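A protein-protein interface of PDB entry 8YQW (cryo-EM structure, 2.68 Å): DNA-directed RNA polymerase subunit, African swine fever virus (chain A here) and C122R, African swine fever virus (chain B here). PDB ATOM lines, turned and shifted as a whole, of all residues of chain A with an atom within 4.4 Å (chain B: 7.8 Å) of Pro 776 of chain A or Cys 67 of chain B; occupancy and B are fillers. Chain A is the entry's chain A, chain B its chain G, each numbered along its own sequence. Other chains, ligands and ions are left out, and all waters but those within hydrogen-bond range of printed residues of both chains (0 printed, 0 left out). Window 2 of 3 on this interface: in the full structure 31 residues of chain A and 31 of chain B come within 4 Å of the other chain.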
ATOM      1  N   GLY A 769     -29.461   2.384  30.934  1.00  0.00           N
ATOM      2  CA  GLY A 769     -29.044   1.181  30.244  1.00  0.00           C
ATOM      3  C   GLY A 769     -28.167   0.264  31.055  1.00  0.00           C
ATOM      4  O   GLY A 769     -27.775  -0.793  30.548  1.00  0.00           O
ATOM      5  N   ARG A 770     -27.839   0.631  32.286  1.00  0.00           N
ATOM      6  CA  ARG A 770     -27.102  -0.227  33.198  1.00  0.00           C
ATOM      7  C   ARG A 770     -28.031  -0.644  34.326  1.00  0.00           C
ATOM      8  O   ARG A 770     -28.748   0.190  34.885  1.00  0.00           O
ATOM      9  CB  ARG A 770     -25.874   0.484  33.762  1.00  0.00           C
ATOM     10  CG  ARG A 770     -25.153   1.367  32.777  1.00  0.00           C
ATOM     11  CD  ARG A 770     -23.900   1.924  33.402  1.00  0.00           C
ATOM     12  NE  ARG A 770     -23.070   0.865  33.958  1.00  0.00           N
ATOM     13  CZ  ARG A 770     -22.098   1.059  34.837  1.00  0.00           C
ATOM     14  NH1 ARG A 770     -21.805   2.266  35.285  1.00  0.00           N
ATOM     15  NH2 ARG A 770     -21.404   0.016  35.276  1.00  0.00           N
ATOM     16  N   TYR A 775     -22.219  -4.132  35.810  1.00  0.00           N
ATOM     17  CA  TYR A 775     -22.437  -4.497  34.426  1.00  0.00           C
ATOM     18  C   TYR A 775     -22.337  -3.269  33.534  1.00  0.00           C
ATOM     19  O   TYR A 775     -22.663  -2.159  33.963  1.00  0.00           O
ATOM     20  CB  TYR A 775     -23.806  -5.157  34.242  1.00  0.00           C
ATOM     21  CG  TYR A 775     -23.979  -6.401  35.074  1.00  0.00           C
ATOM     22  CD1 TYR A 775     -23.300  -7.565  34.757  1.00  0.00           C
ATOM     23  CD2 TYR A 775     -24.809  -6.407  36.184  1.00  0.00           C
ATOM     24  CE1 TYR A 775     -23.447  -8.700  35.515  1.00  0.00           C
ATOM     25  CE2 TYR A 775     -24.963  -7.540  36.946  1.00  0.00           C
ATOM     26  CZ  TYR A 775     -24.278  -8.683  36.607  1.00  0.00           C
ATOM     27  OH  TYR A 775     -24.427  -9.820  37.361  1.00  0.00           O
ATOM     28  N   PRO A 776     -21.886  -3.432  32.294  1.00  0.00           N
ATOM     29  CA  PRO A 776     -21.727  -2.271  31.411  1.00  0.00           C
ATOM     30  C   PRO A 776     -23.054  -1.733  30.913  1.00  0.00           C
ATOM     31  O   PRO A 776     -24.116  -2.273  31.231  1.00  0.00           O
ATOM     32  CB  PRO A 776     -20.880  -2.825  30.262  1.00  0.00           C
ATOM     33  CG  PRO A 776     -21.191  -4.263  30.241  1.00  0.00           C
ATOM     34  CD  PRO A 776     -21.402  -4.669  31.662  1.00  0.00           C
ATOM     35  N   ARG A 777     -23.003  -0.656  30.138  1.00  0.00           N
ATOM     36  CA  ARG A 777     -24.202  -0.096  29.542  1.00  0.00           C
ATOM     37  C   ARG A 777     -24.606  -0.915  28.326  1.00  0.00           C
ATOM     38  O   ARG A 777     -23.757  -1.331  27.533  1.00  0.00           O
ATOM     39  CB  ARG A 777     -23.966   1.360  29.147  1.00  0.00           C
ATOM     40  CG  ARG A 777     -25.229   2.141  28.864  1.00  0.00           C
ATOM     41  CD  ARG A 777     -24.925   3.605  28.646  1.00  0.00           C
ATOM     42  NE  ARG A 777     -24.837   4.333  29.904  1.00  0.00           N
ATOM     43  CZ  ARG A 777     -23.755   4.972  30.322  1.00  0.00           C
ATOM     44  NH1 ARG A 777     -22.649   5.000  29.598  1.00  0.00           N
ATOM     45  NH2 ARG A 777     -23.780   5.594  31.495  1.00  0.00           N
ATOM     46  N   PHE A 778     -25.911  -1.146  28.187  1.00  0.00           N
ATOM     47  CA  PHE A 778     -26.465  -1.953  27.098  1.00  0.00           C
ATOM     48  C   PHE A 778     -25.871  -3.358  27.093  1.00  0.00           C
ATOM     49  O   PHE A 778     -25.636  -3.947  26.037  1.00  0.00           O
ATOM     50  CB  PHE A 778     -26.264  -1.279  25.740  1.00  0.00           C
ATOM     51  CG  PHE A 778     -26.553   0.191  25.743  1.00  0.00           C
ATOM     52  CD1 PHE A 778     -27.787   0.665  26.145  1.00  0.00           C
ATOM     53  CD2 PHE A 778     -25.591   1.097  25.341  1.00  0.00           C
ATOM     54  CE1 PHE A 778     -28.052   2.014  26.149  1.00  0.00           C
ATOM     55  CE2 PHE A 778     -25.853   2.445  25.342  1.00  0.00           C
ATOM     56  CZ  PHE A 778     -27.085   2.904  25.747  1.00  0.00           C
ATOM     57  N   ALA A 779     -25.626  -3.899  28.284  1.00  0.00           N
ATOM     58  CA  ALA A 779     -25.129  -5.262  28.397  1.00  0.00           C
ATOM     59  C   ALA A 779     -26.155  -6.239  27.841  1.00  0.00           C
ATOM     60  O   ALA A 779     -27.362  -6.070  28.025  1.00  0.00           O
ATOM     61  CB  ALA A 779     -24.815  -5.595  29.854  1.00  0.00           C
ATOM     62  N   ALA B  60     -19.572   7.709  22.948  1.00  0.00           N
ATOM     63  CA  ALA B  60     -19.673   6.300  23.321  1.00  0.00           C
ATOM     64  C   ALA B  60     -18.344   5.550  23.311  1.00  0.00           C
ATOM     65  O   ALA B  60     -18.105   4.779  24.255  1.00  0.00           O
ATOM     66  CB  ALA B  60     -20.693   5.602  22.412  1.00  0.00           C
ATOM     67  N   ASP B  63     -16.510   6.325  26.724  1.00  0.00           N
ATOM     68  CA  ASP B  63     -17.112   5.969  27.999  1.00  0.00           C
ATOM     69  C   ASP B  63     -16.677   4.562  28.382  1.00  0.00           C
ATOM     70  O   ASP B  63     -16.942   3.616  27.631  1.00  0.00           O
ATOM     71  CB  ASP B  63     -18.630   6.057  27.907  1.00  0.00           C
ATOM     72  CG  ASP B  63     -19.294   6.100  29.262  1.00  0.00           C
ATOM     73  OD1 ASP B  63     -18.690   6.650  30.203  1.00  0.00           O
ATOM     74  OD2 ASP B  63     -20.424   5.589  29.388  1.00  0.00           O
ATOM     75  N   PRO B  64     -16.010   4.372  29.523  1.00  0.00           N
ATOM     76  CA  PRO B  64     -15.559   3.027  29.900  1.00  0.00           C
ATOM     77  C   PRO B  64     -16.667   2.118  30.397  1.00  0.00           C
ATOM     78  O   PRO B  64     -16.417   0.923  30.599  1.00  0.00           O
ATOM     79  CB  PRO B  64     -14.536   3.303  31.010  1.00  0.00           C
ATOM     80  CG  PRO B  64     -14.965   4.590  31.597  1.00  0.00           C
ATOM     81  CD  PRO B  64     -15.560   5.398  30.479  1.00  0.00           C
ATOM     82  N   THR B  65     -17.874   2.634  30.598  1.00  0.00           N
ATOM     83  CA  THR B  65     -18.989   1.848  31.100  1.00  0.00           C
ATOM     84  C   THR B  65     -19.856   1.273  29.989  1.00  0.00           C
ATOM     85  O   THR B  65     -20.907   0.697  30.279  1.00  0.00           O
ATOM     86  CB  THR B  65     -19.848   2.696  32.038  1.00  0.00           C
ATOM     87  OG1 THR B  65     -20.630   3.616  31.269  1.00  0.00           O
ATOM     88  CG2 THR B  65     -18.971   3.472  32.991  1.00  0.00           C
ATOM     89  N   ASN B  66     -19.446   1.417  28.734  1.00  0.00           N
ATOM     90  CA  ASN B  66     -20.230   0.943  27.605  1.00  0.00           C
ATOM     91  C   ASN B  66     -19.799  -0.460  27.197  1.00  0.00           C
ATOM     92  O   ASN B  66     -18.634  -0.838  27.335  1.00  0.00           O
ATOM     93  CB  ASN B  66     -20.094   1.894  26.417  1.00  0.00           C
ATOM     94  CG  ASN B  66     -20.941   3.131  26.567  1.00  0.00           C
ATOM     95  OD1 ASN B  66     -21.924   3.138  27.304  1.00  0.00           O
ATOM     96  ND2 ASN B  66     -20.573   4.187  25.860  1.00  0.00           N
ATOM     97  N   CYS B  67     -20.760  -1.227  26.690  1.00  0.00           N
ATOM     98  CA  CYS B  67     -20.500  -2.607  26.300  1.00  0.00           C
ATOM     99  C   CYS B  67     -19.564  -2.661  25.102  1.00  0.00           C
ATOM    100  O   CYS B  67     -19.700  -1.881  24.155  1.00  0.00           O
ATOM    101  CB  CYS B  67     -21.812  -3.318  25.974  1.00  0.00           C
ATOM    102  SG  CYS B  67     -21.653  -5.077  25.620  1.00  0.00           S
ATOM    103  N   GLN B  68     -18.612  -3.583  25.143  1.00  0.00           N
ATOM    104  CA  GLN B  68     -17.702  -3.824  24.035  1.00  0.00           C
ATOM    105  C   GLN B  68     -18.042  -5.141  23.353  1.00  0.00           C
ATOM    106  O   GLN B  68     -18.690  -6.018  23.925  1.00  0.00           O
ATOM    107  CB  GLN B  68     -16.251  -3.847  24.515  1.00  0.00           C
ATOM    108  CG  GLN B  68     -15.896  -2.755  25.498  1.00  0.00           C
ATOM    109  CD  GLN B  68     -15.576  -1.449  24.817  1.00  0.00           C
ATOM    110  OE1 GLN B  68     -16.282  -0.460  24.983  1.00  0.00           O
ATOM    111  NE2 GLN B  68     -14.505  -1.440  24.038  1.00  0.00           N
ATOM    112  N   ILE B  69     -17.589  -5.270  22.111  1.00  0.00           N
ATOM    113  CA  ILE B  69     -17.833  -6.461  21.309  1.00  0.00           C
ATOM    114  C   ILE B  69     -16.537  -6.829  20.598  1.00  0.00           C
ATOM    115  O   ILE B  69     -15.778  -5.951  20.176  1.00  0.00           O
ATOM    116  CB  ILE B  69     -18.994  -6.242  20.314  1.00  0.00           C
ATOM    117  CG1 ILE B  69     -19.300  -7.521  19.539  1.00  0.00           C
ATOM    118  CG2 ILE B  69     -18.689  -5.111  19.353  1.00  0.00           C
ATOM    119  CD1 ILE B  69     -20.528  -7.411  18.670  1.00  0.00           C
ATOM    120  N   LEU B  81     -14.975  -3.266  19.185  1.00  0.00           N
ATOM    121  CA  LEU B  81     -15.873  -2.152  18.928  1.00  0.00           C
ATOM    122  C   LEU B  81     -16.757  -1.927  20.145  1.00  0.00           C
ATOM    123  O   LEU B  81     -16.909  -2.802  20.998  1.00  0.00           O
ATOM    124  CB  LEU B  81     -16.746  -2.400  17.691  1.00  0.00           C
ATOM    125  CG  LEU B  81     -16.079  -2.282  16.322  1.00  0.00           C
ATOM    126  CD1 LEU B  81     -17.060  -2.641  15.225  1.00  0.00           C
ATOM    127  CD2 LEU B  81     -15.540  -0.885  16.113  1.00  0.00           C
ATOM    128  N   THR B  82     -17.337  -0.734  20.220  1.00  0.00           N
ATOM    129  CA  THR B  82     -18.286  -0.392  21.271  1.00  0.00           C
ATOM    130  C   THR B  82     -19.695  -0.522  20.711  1.00  0.00           C
ATOM    131  O   THR B  82     -20.038   0.150  19.737  1.00  0.00           O
ATOM    132  CB  THR B  82     -18.043   1.023  21.790  1.00  0.00           C
ATOM    133  OG1 THR B  82     -16.699   1.135  22.270  1.00  0.00           O
ATOM    134  CG2 THR B  82     -19.007   1.346  22.914  1.00  0.00           C
ATOM    135  N   GLN B  83     -20.506  -1.376  21.322  1.00  0.00           N
ATOM    136  CA  GLN B  83     -21.860  -1.621  20.848  1.00  0.00           C
ATOM    137  C   GLN B  83     -22.855  -0.902  21.750  1.00  0.00           C
ATOM    138  O   GLN B  83     -22.753  -0.972  22.977  1.00  0.00           O
ATOM    139  CB  GLN B  83     -22.155  -3.123  20.780  1.00  0.00           C
ATOM    140  CG  GLN B  83     -22.431  -3.818  22.099  1.00  0.00           C
ATOM    141  CD  GLN B  83     -23.914  -3.994  22.361  1.00  0.00           C
ATOM    142  OE1 GLN B  83     -24.701  -4.165  21.433  1.00  0.00           O
ATOM    143  NE2 GLN B  83     -24.301  -3.948  23.629  1.00  0.00           N
ATOM    144  N   ILE B  84     -23.790  -0.177  21.137  1.00  0.00           N
ATOM    145  CA  ILE B  84     -24.841   0.514  21.869  1.00  0.00           C
ATOM    146  C   ILE B  84     -26.182   0.123  21.269  1.00  0.00           C
ATOM    147  O   ILE B  84     -26.289  -0.174  20.076  1.00  0.00           O
ATOM    148  CB  ILE B  84     -24.655   2.050  21.862  1.00  0.00           C
ATOM    149  CG1 ILE B  84     -24.875   2.626  20.467  1.00  0.00           C
ATOM    150  CG2 ILE B  84     -23.273   2.429  22.359  1.00  0.00           C
ATOM    151  CD1 ILE B  84     -24.639   4.108  20.391  1.00  0.00           C
ATOM    152  N   CYS B  85     -27.211   0.108  22.112  1.00  0.00           N
ATOM    153  CA  CYS B  85     -28.552  -0.323  21.724  1.00  0.00           C
ATOM    154  C   CYS B  85     -29.532   0.762  22.154  1.00  0.00           C
ATOM    155  O   CYS B  85     -29.852   0.882  23.340  1.00  0.00           O
ATOM    156  CB  CYS B  85     -28.895  -1.669  22.352  1.00  0.00           C
ATOM    157  SG  CYS B  85     -30.492  -2.342  21.866  1.00  0.00           S
ATOM    158  N   ILE B  93     -25.788   0.041  17.233  1.00  0.00           N
ATOM    159  CA  ILE B  93     -24.778   0.856  16.572  1.00  0.00           C
ATOM    160  C   ILE B  93     -23.414   0.470  17.124  1.00  0.00           C
ATOM    161  O   ILE B  93     -23.221   0.435  18.344  1.00  0.00           O
ATOM    162  CB  ILE B  93     -25.034   2.362  16.768  1.00  0.00           C
ATOM    163  CG1 ILE B  93     -26.411   2.744  16.228  1.00  0.00           C
ATOM    164  CG2 ILE B  93     -23.954   3.183  16.089  1.00  0.00           C
ATOM    165  CD1 ILE B  93     -26.889   4.090  16.698  1.00  0.00           C
ATOM    166  N   LEU B  94     -22.478   0.175  16.229  1.00  0.00           N
ATOM    167  CA  LEU B  94     -21.100  -0.107  16.596  1.00  0.00           C
ATOM    168  C   LEU B  94     -20.257   1.125  16.309  1.00  0.00           C
ATOM    169  O   LEU B  94     -20.324   1.685  15.212  1.00  0.00           O
ATOM    170  CB  LEU B  94     -20.558  -1.311  15.824  1.00  0.00           C
ATOM    171  CG  LEU B  94     -21.398  -2.586  15.839  1.00  0.00           C
ATOM    172  CD1 LEU B  94     -20.631  -3.728  15.208  1.00  0.00           C
ATOM    173  CD2 LEU B  94     -21.815  -2.943  17.251  1.00  0.00           C
ATOM    174  N   VAL B  95     -19.469   1.545  17.294  1.00  0.00           N
ATOM    175  CA  VAL B  95     -18.673   2.757  17.200  1.00  0.00           C
ATOM    176  C   VAL B  95     -17.244   2.444  17.620  1.00  0.00           C
ATOM    177  O   VAL B  95     -16.978   1.483  18.345  1.00  0.00           O
ATOM    178  CB  VAL B  95     -19.253   3.902  18.059  1.00  0.00           C
ATOM    179  CG1 VAL B  95     -20.543   4.409  17.460  1.00  0.00           C
ATOM    180  CG2 VAL B  95     -19.497   3.427  19.470  1.00  0.00           C
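OD2 of Asp 63 of chain B lies within salt-bridge range of NH2 of Arg 777 of chain A. The backbone carbonyl oxygen (O) of Thr 65 of chain B sits at hydrogen-bond distance from the backbone NH (N) of Arg 777 of chain A, 2.5 Å away. The guanidinium group of Arg 777 of chain A is in hydrogen-bond range of the side-chain amide oxygen of Asn 66 of chain B (3.0 Å). O of Arg 777 of chain A is in hydrogen-bond range of N of Cys 67 of chain B, 3.1 Å away. The backbone carbonyl oxygen of Phe 778 of chain A is in hydrogen-bond range of the side-chain amide nitrogen of Gln 83 of chain B (2.8 Å).
O of Gly 769 of chain A sits at hydrogen-bond distance from N of Phe 778 of chain A (3.0 Å). O of Ala 60 of chain B is in hydrogen-bond range of ND2 of Asn 66 of chain B (3.0 Å). OD2 of Asp 63 of chain B sits at hydrogen-bond distance from OG1 of Thr 65 of chain B. OE1 of Gln 68 of chain B sits close to O of Asn 66 of chain B, 3.3 Å away. O of Cys 67 of chain B sits at hydrogen-bond distance from N of Gln 83 of chain B. The backbone NH (N) of Ile 93 of chain B is in hydrogen-bond range of the backbone carbonyl oxygen (O) of Ile 84 of chain B.
Among the printed residues, pairs that only touch across the chains: Pro 776 of chain A with Thr 65 of chain B (3.3 Å), Phe 778 of chain A with Cys 85 of chain B (3.5 Å), Phe 778 of chain A with Ile 84 of chain B (3.6 Å), Arg 770 of chain A with Thr 65 of chain B (3.8 Å), Phe 778 of chain A with Cys 67 of chain B (3.9 Å) and Pro 776 of chain A with Cys 67 of chain B (3.9 Å).
Of the printed residues of chain B, Pro 776 of chain A touches Thr 65 (3.3 Å) and Cys 67 (3.9 Å). Of the printed residues of chain A, Asn 66 of chain B touches Arg 777 (3.0 Å). Cys 67 of chain B touches just these residues of chain A: Pro 776 (3.9 Å), Arg 777 (3.1 Å) and Phe 778 (3.9 Å). Of the printed residues of chain A, Gln 83 of chain B touches Phe 778 (2.8 Å). The nearest printed residue of chain B that does not touch Pro 776 of chain A is Asn 66 of chain B (4.02 Å). The nearest printed residue of chain A that does not touch Asp 63 of chain B is Arg 770 of chain A (6.5 Å).
Of the 16 printed residues of chain B, 7 touch a printed residue of chain A. Printed residues of chain A that touch a printed residue of chain B: Arg 770, Pro 776, Arg 777 and Phe 778. Hydrophobic or aromatic side chains of chain A within 4 Å of the printed part of chain B: Pro 776 and Phe 778.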
